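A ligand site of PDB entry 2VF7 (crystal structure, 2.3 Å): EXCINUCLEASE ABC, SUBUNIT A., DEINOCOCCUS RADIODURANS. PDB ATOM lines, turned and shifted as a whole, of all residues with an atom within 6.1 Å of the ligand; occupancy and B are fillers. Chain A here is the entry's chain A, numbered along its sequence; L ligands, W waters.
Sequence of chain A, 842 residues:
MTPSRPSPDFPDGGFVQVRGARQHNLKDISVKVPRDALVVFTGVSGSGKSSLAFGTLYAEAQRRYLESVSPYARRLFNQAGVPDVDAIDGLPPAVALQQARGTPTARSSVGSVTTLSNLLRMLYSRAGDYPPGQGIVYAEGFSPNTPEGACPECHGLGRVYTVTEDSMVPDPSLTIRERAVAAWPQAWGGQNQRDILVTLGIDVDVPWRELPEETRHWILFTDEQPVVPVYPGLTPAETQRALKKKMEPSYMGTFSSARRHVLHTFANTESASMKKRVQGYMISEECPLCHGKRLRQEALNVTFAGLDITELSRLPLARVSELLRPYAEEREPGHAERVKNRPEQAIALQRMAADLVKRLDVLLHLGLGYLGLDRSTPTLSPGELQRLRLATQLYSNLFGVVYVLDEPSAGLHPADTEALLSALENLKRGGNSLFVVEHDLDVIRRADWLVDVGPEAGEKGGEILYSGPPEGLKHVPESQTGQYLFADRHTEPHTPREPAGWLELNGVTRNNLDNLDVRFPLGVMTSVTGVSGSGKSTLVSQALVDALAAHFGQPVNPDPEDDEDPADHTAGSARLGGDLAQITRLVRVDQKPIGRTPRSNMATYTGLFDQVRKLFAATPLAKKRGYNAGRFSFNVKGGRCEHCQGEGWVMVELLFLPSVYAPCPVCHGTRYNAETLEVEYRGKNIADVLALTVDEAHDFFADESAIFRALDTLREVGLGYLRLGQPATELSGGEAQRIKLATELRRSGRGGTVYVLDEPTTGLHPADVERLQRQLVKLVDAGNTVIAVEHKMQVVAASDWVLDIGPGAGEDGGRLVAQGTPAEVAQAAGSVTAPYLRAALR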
ATOM      1  N   TYR A 370       3.635 -26.728  14.887  1.00  0.00           N
ATOM      2  CA  TYR A 370       4.769 -26.525  15.809  1.00  0.00           C
ATOM      3  C   TYR A 370       5.474 -25.189  15.551  1.00  0.00           C
ATOM      4  O   TYR A 370       6.337 -24.761  16.331  1.00  0.00           O
ATOM      5  CB  TYR A 370       5.775 -27.686  15.698  1.00  0.00           C
ATOM      6  CG  TYR A 370       6.368 -27.829  14.310  1.00  0.00           C
ATOM      7  CD1 TYR A 370       5.775 -28.653  13.342  1.00  0.00           C
ATOM      8  CD2 TYR A 370       7.517 -27.125  13.957  1.00  0.00           C
ATOM      9  CE1 TYR A 370       6.321 -28.765  12.051  1.00  0.00           C
ATOM     10  CE2 TYR A 370       8.062 -27.235  12.685  1.00  0.00           C
ATOM     11  CZ  TYR A 370       7.459 -28.051  11.747  1.00  0.00           C
ATOM     12  OH  TYR A 370       8.034 -28.136  10.503  1.00  0.00           O
ATOM     13  N   LEU A 371       5.110 -24.533  14.444  1.00  0.00           N
ATOM     14  CA  LEU A 371       5.638 -23.229  14.078  1.00  0.00           C
ATOM     15  C   LEU A 371       4.913 -22.106  14.812  1.00  0.00           C
ATOM     16  O   LEU A 371       3.728 -22.202  15.096  1.00  0.00           O
ATOM     17  CB  LEU A 371       5.516 -23.019  12.557  1.00  0.00           C
ATOM     18  CG  LEU A 371       6.347 -23.917  11.622  1.00  0.00           C
ATOM     19  CD1 LEU A 371       6.012 -23.696  10.148  1.00  0.00           C
ATOM     20  CD2 LEU A 371       7.841 -23.744  11.856  1.00  0.00           C
ATOM     21  N   GLY A 372       5.639 -21.030  15.113  1.00  0.00           N
ATOM     22  CA  GLY A 372       5.051 -19.844  15.740  1.00  0.00           C
ATOM     23  C   GLY A 372       4.802 -18.784  14.682  1.00  0.00           C
ATOM     24  O   GLY A 372       5.560 -18.677  13.717  1.00  0.00           O
ATOM     25  N   ARG A 375       7.637 -16.472  13.459  1.00  0.00           N
ATOM     26  CA  ARG A 375       8.775 -17.154  12.853  1.00  0.00           C
ATOM     27  C   ARG A 375       9.058 -16.642  11.448  1.00  0.00           C
ATOM     28  O   ARG A 375       8.164 -16.594  10.586  1.00  0.00           O
ATOM     29  CB  ARG A 375       8.491 -18.664  12.835  1.00  0.00           C
ATOM     30  CG  ARG A 375       9.458 -19.519  12.047  1.00  0.00           C
ATOM     31  CD  ARG A 375      10.691 -19.843  12.847  1.00  0.00           C
ATOM     32  NE  ARG A 375      11.576 -20.736  12.115  1.00  0.00           N
ATOM     33  CZ  ARG A 375      11.610 -22.056  12.256  1.00  0.00           C
ATOM     34  NH1 ARG A 375      10.791 -22.661  13.104  1.00  0.00           N
ATOM     35  NH2 ARG A 375      12.455 -22.771  11.530  1.00  0.00           N
ATOM     36  N   THR A 379      14.230 -18.570   7.914  1.00  0.00           N
ATOM     37  CA  THR A 379      14.701 -19.565   8.875  1.00  0.00           C
ATOM     38  C   THR A 379      13.999 -20.908   8.670  1.00  0.00           C
ATOM     39  O   THR A 379      14.250 -21.871   9.393  1.00  0.00           O
ATOM     40  CB  THR A 379      14.540 -19.082  10.334  1.00  0.00           C
ATOM     41  OG1 THR A 379      13.164 -19.103  10.717  1.00  0.00           O
ATOM     42  CG2 THR A 379      15.115 -17.684  10.510  1.00  0.00           C
ATOM     43  N   GLU A 384       9.236 -26.747   4.404  1.00  0.00           N
ATOM     44  CA  GLU A 384       8.358 -26.088   5.358  1.00  0.00           C
ATOM     45  C   GLU A 384       7.529 -24.973   4.701  1.00  0.00           C
ATOM     46  O   GLU A 384       6.305 -25.001   4.805  1.00  0.00           O
ATOM     47  CB  GLU A 384       9.138 -25.585   6.571  1.00  0.00           C
ATOM     48  CG  GLU A 384       9.144 -26.590   7.751  1.00  0.00           C
ATOM     49  CD  GLU A 384      10.138 -26.244   8.875  1.00  0.00           C
ATOM     50  OE1 GLU A 384      11.005 -25.381   8.680  1.00  0.00           O
ATOM     51  OE2 GLU A 384      10.055 -26.873   9.954  1.00  0.00           O
ATOM     52  N   GLY A 411      11.665 -33.166   3.456  1.00  0.00           N
ATOM     53  CA  GLY A 411      11.648 -32.903   4.884  1.00  0.00           C
ATOM     54  C   GLY A 411      10.478 -33.556   5.573  1.00  0.00           C
ATOM     55  O   GLY A 411      10.286 -33.395   6.781  1.00  0.00           O
ATOM     56  N   ARG A 510      17.660 -25.554  23.901  1.00  0.00           N
ATOM     57  CA  ARG A 510      17.465 -24.902  22.594  1.00  0.00           C
ATOM     58  C   ARG A 510      16.074 -25.251  22.042  1.00  0.00           C
ATOM     59  O   ARG A 510      15.732 -26.426  21.859  1.00  0.00           O
ATOM     60  CB  ARG A 510      18.551 -25.354  21.604  1.00  0.00           C
ATOM     61  CG  ARG A 510      18.738 -24.470  20.382  1.00  0.00           C
ATOM     62  CD  ARG A 510      20.222 -24.134  20.171  1.00  0.00           C
ATOM     63  NE  ARG A 510      20.425 -23.283  18.993  1.00  0.00           N
ATOM     64  CZ  ARG A 510      21.453 -22.444  18.833  1.00  0.00           C
ATOM     65  NH1 ARG A 510      22.380 -22.333  19.775  1.00  0.00           N
ATOM     66  NH2 ARG A 510      21.543 -21.715  17.720  1.00  0.00           N
ATOM     67  N   ASN A 511      15.268 -24.210  21.798  1.00  0.00           N
ATOM     68  CA  ASN A 511      13.915 -24.366  21.271  1.00  0.00           C
ATOM     69  C   ASN A 511      13.100 -25.365  22.080  1.00  0.00           C
ATOM     70  O   ASN A 511      12.753 -25.089  23.220  1.00  0.00           O
ATOM     71  CB  ASN A 511      13.954 -24.753  19.779  1.00  0.00           C
ATOM     72  CG  ASN A 511      14.671 -23.732  18.937  1.00  0.00           C
ATOM     73  OD1 ASN A 511      14.885 -22.607  19.357  1.00  0.00           O
ATOM     74  ND2 ASN A 511      15.035 -24.121  17.720  1.00  0.00           N
ATOM     75  N   ASN A 512      12.821 -26.549  21.505  1.00  0.00           N
ATOM     76  CA  ASN A 512      12.028 -27.593  22.198  1.00  0.00           C
ATOM     77  C   ASN A 512      12.805 -28.686  22.963  1.00  0.00           C
ATOM     78  O   ASN A 512      12.203 -29.616  23.502  1.00  0.00           O
ATOM     79  CB  ASN A 512      10.968 -28.203  21.259  1.00  0.00           C
ATOM     80  CG  ASN A 512      11.550 -29.175  20.261  1.00  0.00           C
ATOM     81  OD1 ASN A 512      12.674 -29.016  19.787  1.00  0.00           O
ATOM     82  ND2 ASN A 512      10.767 -30.184  19.901  1.00  0.00           N
ATOM     83  N   GLY A 530      13.267 -38.789  12.694  1.00  0.00           N
ATOM     84  CA  GLY A 530      12.185 -38.213  13.486  1.00  0.00           C
ATOM     85  C   GLY A 530      11.222 -37.368  12.672  1.00  0.00           C
ATOM     86  O   GLY A 530      11.554 -36.937  11.550  1.00  0.00           O
ATOM     87  N   VAL A 531      10.032 -37.146  13.237  1.00  0.00           N
ATOM     88  CA  VAL A 531       8.945 -36.309  12.674  1.00  0.00           C
ATOM     89  C   VAL A 531       9.395 -34.857  12.388  1.00  0.00           C
ATOM     90  O   VAL A 531      10.370 -34.385  13.002  1.00  0.00           O
ATOM     91  CB  VAL A 531       7.710 -36.372  13.659  1.00  0.00           C
ATOM     92  CG1 VAL A 531       7.032 -35.032  13.871  1.00  0.00           C
ATOM     93  CG2 VAL A 531       6.719 -37.459  13.246  1.00  0.00           C
ATOM     94  N   SER A 532       8.726 -34.159  11.464  1.00  0.00           N
ATOM     95  CA  SER A 532       9.038 -32.761  11.195  1.00  0.00           C
ATOM     96  C   SER A 532       8.725 -31.945  12.447  1.00  0.00           C
ATOM     97  O   SER A 532       7.687 -32.138  13.078  1.00  0.00           O
ATOM     98  CB  SER A 532       8.237 -32.195  10.024  1.00  0.00           C
ATOM     99  OG  SER A 532       8.176 -33.126   8.955  1.00  0.00           O
ATOM    100  N   GLY A 533       9.631 -31.039  12.791  1.00  0.00           N
ATOM    101  CA  GLY A 533       9.466 -30.230  14.006  1.00  0.00           C
ATOM    102  C   GLY A 533       9.839 -30.952  15.293  1.00  0.00           C
ATOM    103  O   GLY A 533       9.596 -30.431  16.383  1.00  0.00           O
ATOM    104  N   SER A 534      10.416 -32.149  15.152  1.00  0.00           N
ATOM    105  CA  SER A 534      10.947 -32.928  16.287  1.00  0.00           C
ATOM    106  C   SER A 534      12.093 -32.239  17.004  1.00  0.00           C
ATOM    107  O   SER A 534      12.005 -32.000  18.203  1.00  0.00           O
ATOM    108  CB  SER A 534      11.441 -34.287  15.802  1.00  0.00           C
ATOM    109  OG  SER A 534      10.357 -35.081  15.381  1.00  0.00           O
ATOM    110  N   GLY A 535      13.161 -31.951  16.271  1.00  0.00           N
ATOM    111  CA  GLY A 535      14.348 -31.315  16.865  1.00  0.00           C
ATOM    112  C   GLY A 535      15.680 -31.782  16.323  1.00  0.00           C
ATOM    113  O   GLY A 535      16.722 -31.402  16.838  1.00  0.00           O
ATOM    114  N   LYS A 536      15.648 -32.602  15.280  1.00  0.00           N
ATOM    115  CA  LYS A 536      16.850 -33.123  14.602  1.00  0.00           C
ATOM    116  C   LYS A 536      17.775 -32.005  14.133  1.00  0.00           C
ATOM    117  O   LYS A 536      18.969 -31.964  14.461  1.00  0.00           O
ATOM    118  CB  LYS A 536      16.417 -33.934  13.362  1.00  0.00           C
ATOM    119  CG  LYS A 536      15.114 -34.680  13.518  1.00  0.00           C
ATOM    120  CD  LYS A 536      14.855 -35.481  12.278  1.00  0.00           C
ATOM    121  CE  LYS A 536      14.366 -34.624  11.114  1.00  0.00           C
ATOM    122  NZ  LYS A 536      12.960 -34.202  11.338  1.00  0.00           N
ATOM    123  N   SER A 537      17.203 -31.111  13.345  1.00  0.00           N
ATOM    124  CA  SER A 537      17.871 -29.901  12.912  1.00  0.00           C
ATOM    125  C   SER A 537      18.362 -29.034  14.084  1.00  0.00           C
ATOM    126  O   SER A 537      19.460 -28.478  14.032  1.00  0.00           O
ATOM    127  CB  SER A 537      16.967 -29.155  11.919  1.00  0.00           C
ATOM    128  OG  SER A 537      17.132 -27.755  11.990  1.00  0.00           O
ATOM    129  N   THR A 538      17.562 -28.951  15.145  1.00  0.00           N
ATOM    130  CA  THR A 538      17.914 -28.220  16.364  1.00  0.00           C
ATOM    131  C   THR A 538      19.061 -28.893  17.128  1.00  0.00           C
ATOM    132  O   THR A 538      19.914 -28.209  17.693  1.00  0.00           O
ATOM    133  CB  THR A 538      16.702 -28.026  17.316  1.00  0.00           C
ATOM    134  OG1 THR A 538      15.553 -27.642  16.560  1.00  0.00           O
ATOM    135  CG2 THR A 538      16.962 -26.942  18.327  1.00  0.00           C
ATOM    136  N   LEU A 539      19.074 -30.232  17.141  1.00  0.00           N
ATOM    137  CA  LEU A 539      20.151 -31.006  17.756  1.00  0.00           C
ATOM    138  C   LEU A 539      21.434 -31.016  16.932  1.00  0.00           C
ATOM    139  O   LEU A 539      22.508 -30.723  17.449  1.00  0.00           O
ATOM    140  CB  LEU A 539      19.698 -32.436  18.029  1.00  0.00           C
ATOM    141  CG  LEU A 539      20.687 -33.407  18.689  1.00  0.00           C
ATOM    142  CD1 LEU A 539      20.967 -33.061  20.139  1.00  0.00           C
ATOM    143  CD2 LEU A 539      20.164 -34.827  18.586  1.00  0.00           C
ATOM    144  N   GLN A 542      22.085 -27.075  14.449  1.00  0.00           N
ATOM    145  CA  GLN A 542      22.264 -25.940  15.352  1.00  0.00           C
ATOM    146  C   GLN A 542      23.152 -26.266  16.552  1.00  0.00           C
ATOM    147  O   GLN A 542      24.240 -25.740  16.655  1.00  0.00           O
ATOM    148  CB  GLN A 542      20.913 -25.343  15.756  1.00  0.00           C
ATOM    149  CG  GLN A 542      20.060 -24.925  14.544  1.00  0.00           C
ATOM    150  CD  GLN A 542      18.650 -24.492  14.918  1.00  0.00           C
ATOM    151  OE1 GLN A 542      18.454 -23.824  15.949  1.00  0.00           O
ATOM    152  NE2 GLN A 542      17.669 -24.869  14.101  1.00  0.00           N
ATOM    153  N   VAL A 789      21.400 -35.590   9.288  1.00  0.00           N
ATOM    154  CA  VAL A 789      19.957 -35.496   9.524  1.00  0.00           C
ATOM    155  C   VAL A 789      19.200 -36.000   8.292  1.00  0.00           C
ATOM    156  O   VAL A 789      19.422 -35.547   7.176  1.00  0.00           O
ATOM    157  CB  VAL A 789      19.496 -34.101  10.055  1.00  0.00           C
ATOM    158  CG1 VAL A 789      20.626 -33.083  10.003  1.00  0.00           C
ATOM    159  CG2 VAL A 789      18.182 -33.598   9.402  1.00  0.00           C
ATOM    160  N   HIS A 791      15.693 -38.165   6.363  1.00  0.00           N
ATOM    161  CA  HIS A 791      14.231 -38.286   6.284  1.00  0.00           C
ATOM    162  C   HIS A 791      13.762 -39.520   5.513  1.00  0.00           C
ATOM    163  O   HIS A 791      12.609 -39.928   5.636  1.00  0.00           O
ATOM    164  CB  HIS A 791      13.603 -37.029   5.651  1.00  0.00           C
ATOM    165  CG  HIS A 791      13.954 -35.749   6.355  1.00  0.00           C
ATOM    166  ND1 HIS A 791      14.988 -34.934   5.936  1.00  0.00           N
ATOM    167  CD2 HIS A 791      13.417 -35.159   7.443  1.00  0.00           C
ATOM    168  CE1 HIS A 791      15.072 -33.894   6.749  1.00  0.00           C
ATOM    169  NE2 HIS A 791      14.125 -34.000   7.662  1.00  0.00           N
ATOM    170  N   ALA A 809       6.022 -33.441  17.195  1.00  0.00           N
ATOM    171  CA  ALA A 809       6.622 -32.173  16.844  1.00  0.00           C
ATOM    172  C   ALA A 809       6.475 -31.186  17.985  1.00  0.00           C
ATOM    173  O   ALA A 809       5.578 -31.343  18.814  1.00  0.00           O
ATOM    174  CB  ALA A 809       5.964 -31.637  15.608  1.00  0.00           C
ATOM    175  N   GLY A 810       7.348 -30.189  18.014  1.00  0.00           N
ATOM    176  CA  GLY A 810       7.253 -29.064  18.956  1.00  0.00           C
ATOM    177  C   GLY A 810       7.300 -29.457  20.420  1.00  0.00           C
ATOM    178  O   GLY A 810       8.273 -30.071  20.872  1.00  0.00           O
ATOM    179  N   GLU A 811       6.249 -29.092  21.169  1.00  0.00           N
ATOM    180  CA  GLU A 811       6.124 -29.435  22.594  1.00  0.00           C
ATOM    181  C   GLU A 811       5.989 -30.941  22.799  1.00  0.00           C
ATOM    182  O   GLU A 811       6.460 -31.500  23.804  1.00  0.00           O
ATOM    183  CB  GLU A 811       4.943 -28.691  23.223  1.00  0.00           C
ATOM    184  CG  GLU A 811       5.323 -27.459  24.054  1.00  0.00           C
ATOM    185  CD  GLU A 811       5.195 -27.681  25.575  1.00  0.00           C
ATOM    186  OE1 GLU A 811       4.185 -28.286  26.017  1.00  0.00           O
ATOM    187  OE2 GLU A 811       6.081 -27.222  26.330  1.00  0.00           O
HETATM  188  P1  LIG L   1      13.034 -30.657  12.582  1.00  0.00           P
HETATM  189  O1  LIG L   1      11.981 -30.345  11.543  1.00  0.00           O
HETATM  190  O2  LIG L   1      14.442 -30.290  12.224  1.00  0.00           O
HETATM  191  O3  LIG L   1      12.867 -32.057  13.105  1.00  0.00           O
HETATM  192  P2  LIG L   1      13.508 -28.350  14.273  1.00  0.00           P
HETATM  193  O4  LIG L   1      13.050 -27.180  13.461  1.00  0.00           O
HETATM  194  O5  LIG L   1      14.953 -28.667  14.408  1.00  0.00           O
HETATM  195  O6  LIG L   1      12.705 -29.683  13.844  1.00  0.00           O
HETATM  196  O7  LIG L   1      12.990 -28.018  15.768  1.00  0.00           O
HETATM  197  C1  LIG L   1      11.633 -28.186  16.150  1.00  0.00           C
HETATM  198  C2  LIG L   1      11.128 -27.100  17.093  1.00  0.00           C
HETATM  199  O8  LIG L   1      12.065 -26.029  17.215  1.00  0.00           O
HETATM  200  C3  LIG L   1       9.877 -26.505  16.500  1.00  0.00           C
HETATM  201  O9  LIG L   1       8.940 -26.223  17.533  1.00  0.00           O
HETATM  202  C4  LIG L   1      10.349 -25.228  15.834  1.00  0.00           C
HETATM  203  O10 LIG L   1       9.319 -24.231  15.684  1.00  0.00           O
HETATM  204  C5  LIG L   1      11.482 -24.800  16.747  1.00  0.00           C
HETATM  205  N1  LIG L   1      12.473 -23.979  15.994  1.00  0.00           N
HETATM  206  C6  LIG L   1      13.423 -24.457  15.157  1.00  0.00           C
HETATM  207  N2  LIG L   1      14.167 -23.460  14.631  1.00  0.00           N
HETATM  208  C7  LIG L   1      13.671 -22.303  15.131  1.00  0.00           C
HETATM  209  C8  LIG L   1      13.993 -20.859  14.997  1.00  0.00           C
HETATM  210  N3  LIG L   1      15.000 -20.461  14.188  1.00  0.00           N
HETATM  211  N4  LIG L   1      13.247 -19.969  15.701  1.00  0.00           N
HETATM  212  C9  LIG L   1      12.221 -20.362  16.499  1.00  0.00           C
HETATM  213  N5  LIG L   1      11.889 -21.657  16.674  1.00  0.00           N
HETATM  214  C10 LIG L   1      12.560 -22.650  16.033  1.00  0.00           C
HETATM  215  O   HOH W   1      13.133 -20.790  19.770  1.00  0.00           O
HETATM  216  O   HOH W   2       8.646 -20.583  16.273  1.00  0.00           O
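The backbone NH (N) of Thr 538 sits at hydrogen-bond distance from an oxygen (O5) of the ligand.
An oxygen (O5) of the ligand is in hydrogen-bond range of the side-chain hydroxyl (OG1) of Thr 538, at 2.5 Å.
N of Gly 533 lies within hydrogen-bond range of O1 of the ligand (2.7 Å).
NZ of Lys 536 lies within salt-bridge range of O3 of the ligand, at 2.8 Å.
An oxygen (O2) of the ligand lies close to the backbone NH of Ser 537 (3.1 Å).
The side-chain hydroxyl (OG) of Ser 537 sits close to an oxygen (O5) of the ligand, 3.4 Å away.
A nitrogen (N2) of the ligand lies close to the side-chain amide nitrogen (ND2) of Asn 511, 3.3 Å away.
An oxygen (O10) of the ligand sits at hydrogen-bond distance from the backbone carbonyl oxygen of Tyr 370 (3.1 Å).
The backbone NH (N) of Gly 535 sits at hydrogen-bond distance from an oxygen (O3) of the ligand, 3.2 Å away.
An oxygen (O3) of the ligand lies within hydrogen-bond range of the backbone NH (N) of Ser 534, at 3.2 Å.
The guanidinium group (NH1) of Arg 375 lies within hydrogen-bond range of an oxygen (O10) of the ligand, 3.4 Å away.
The backbone carbonyl oxygen (O) of Gly 533 lies within hydrogen-bond range of the backbone NH (N) of Gly 810 (2.8 Å).
NZ of Lys 536 lies within hydrogen-bond range of O of Gly 530.
N of Gln 542 sits at hydrogen-bond distance from O of Ser 537 (3.0 Å).
OE2 of Glu 384 sits at hydrogen-bond distance from OH of Tyr 370 (2.4 Å).
The side-chain hydroxyl (OG) of Ser 534 lies within hydrogen-bond range of the backbone carbonyl oxygen (O) of Val 531 (2.5 Å).
O of Ser 534 lies within hydrogen-bond range of ND2 of Asn 512.
The backbone carbonyl oxygen (O) of Gly 810 is in hydrogen-bond range of the side-chain amide nitrogen (ND2) of Asn 512 (2.7 Å).
OG of Ser 532 sits at hydrogen-bond distance from O of Gly 411 (3.0 Å).
An oxygen (O3) of the ligand lies close to the backbone carbonyl oxygen (O) of Val 531 (3.4 Å).
Asn 512 touches the ligand (OD1 to C2, 3.6 Å).
C of Ser 532 touches O1 of the ligand (3.7 Å).
Gln 542 touches the ligand (NE2 to N2, 3.8 Å).
Gly 810 touches the ligand.
Hydrophobic or aromatic side chains that line the ligand: Tyr 370.
Of the 26 residues printed, 14 come within 4 Å of the ligand.
Water W1 bridges the side-chain amide oxygen of Asn 511 (2.6 Å) and a nitrogen (N5) of the ligand (3.4 Å).
Water W2 lies within hydrogen-bond range of N of Gly 372 (3.3 Å) and N5 of the ligand (3.4 Å).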
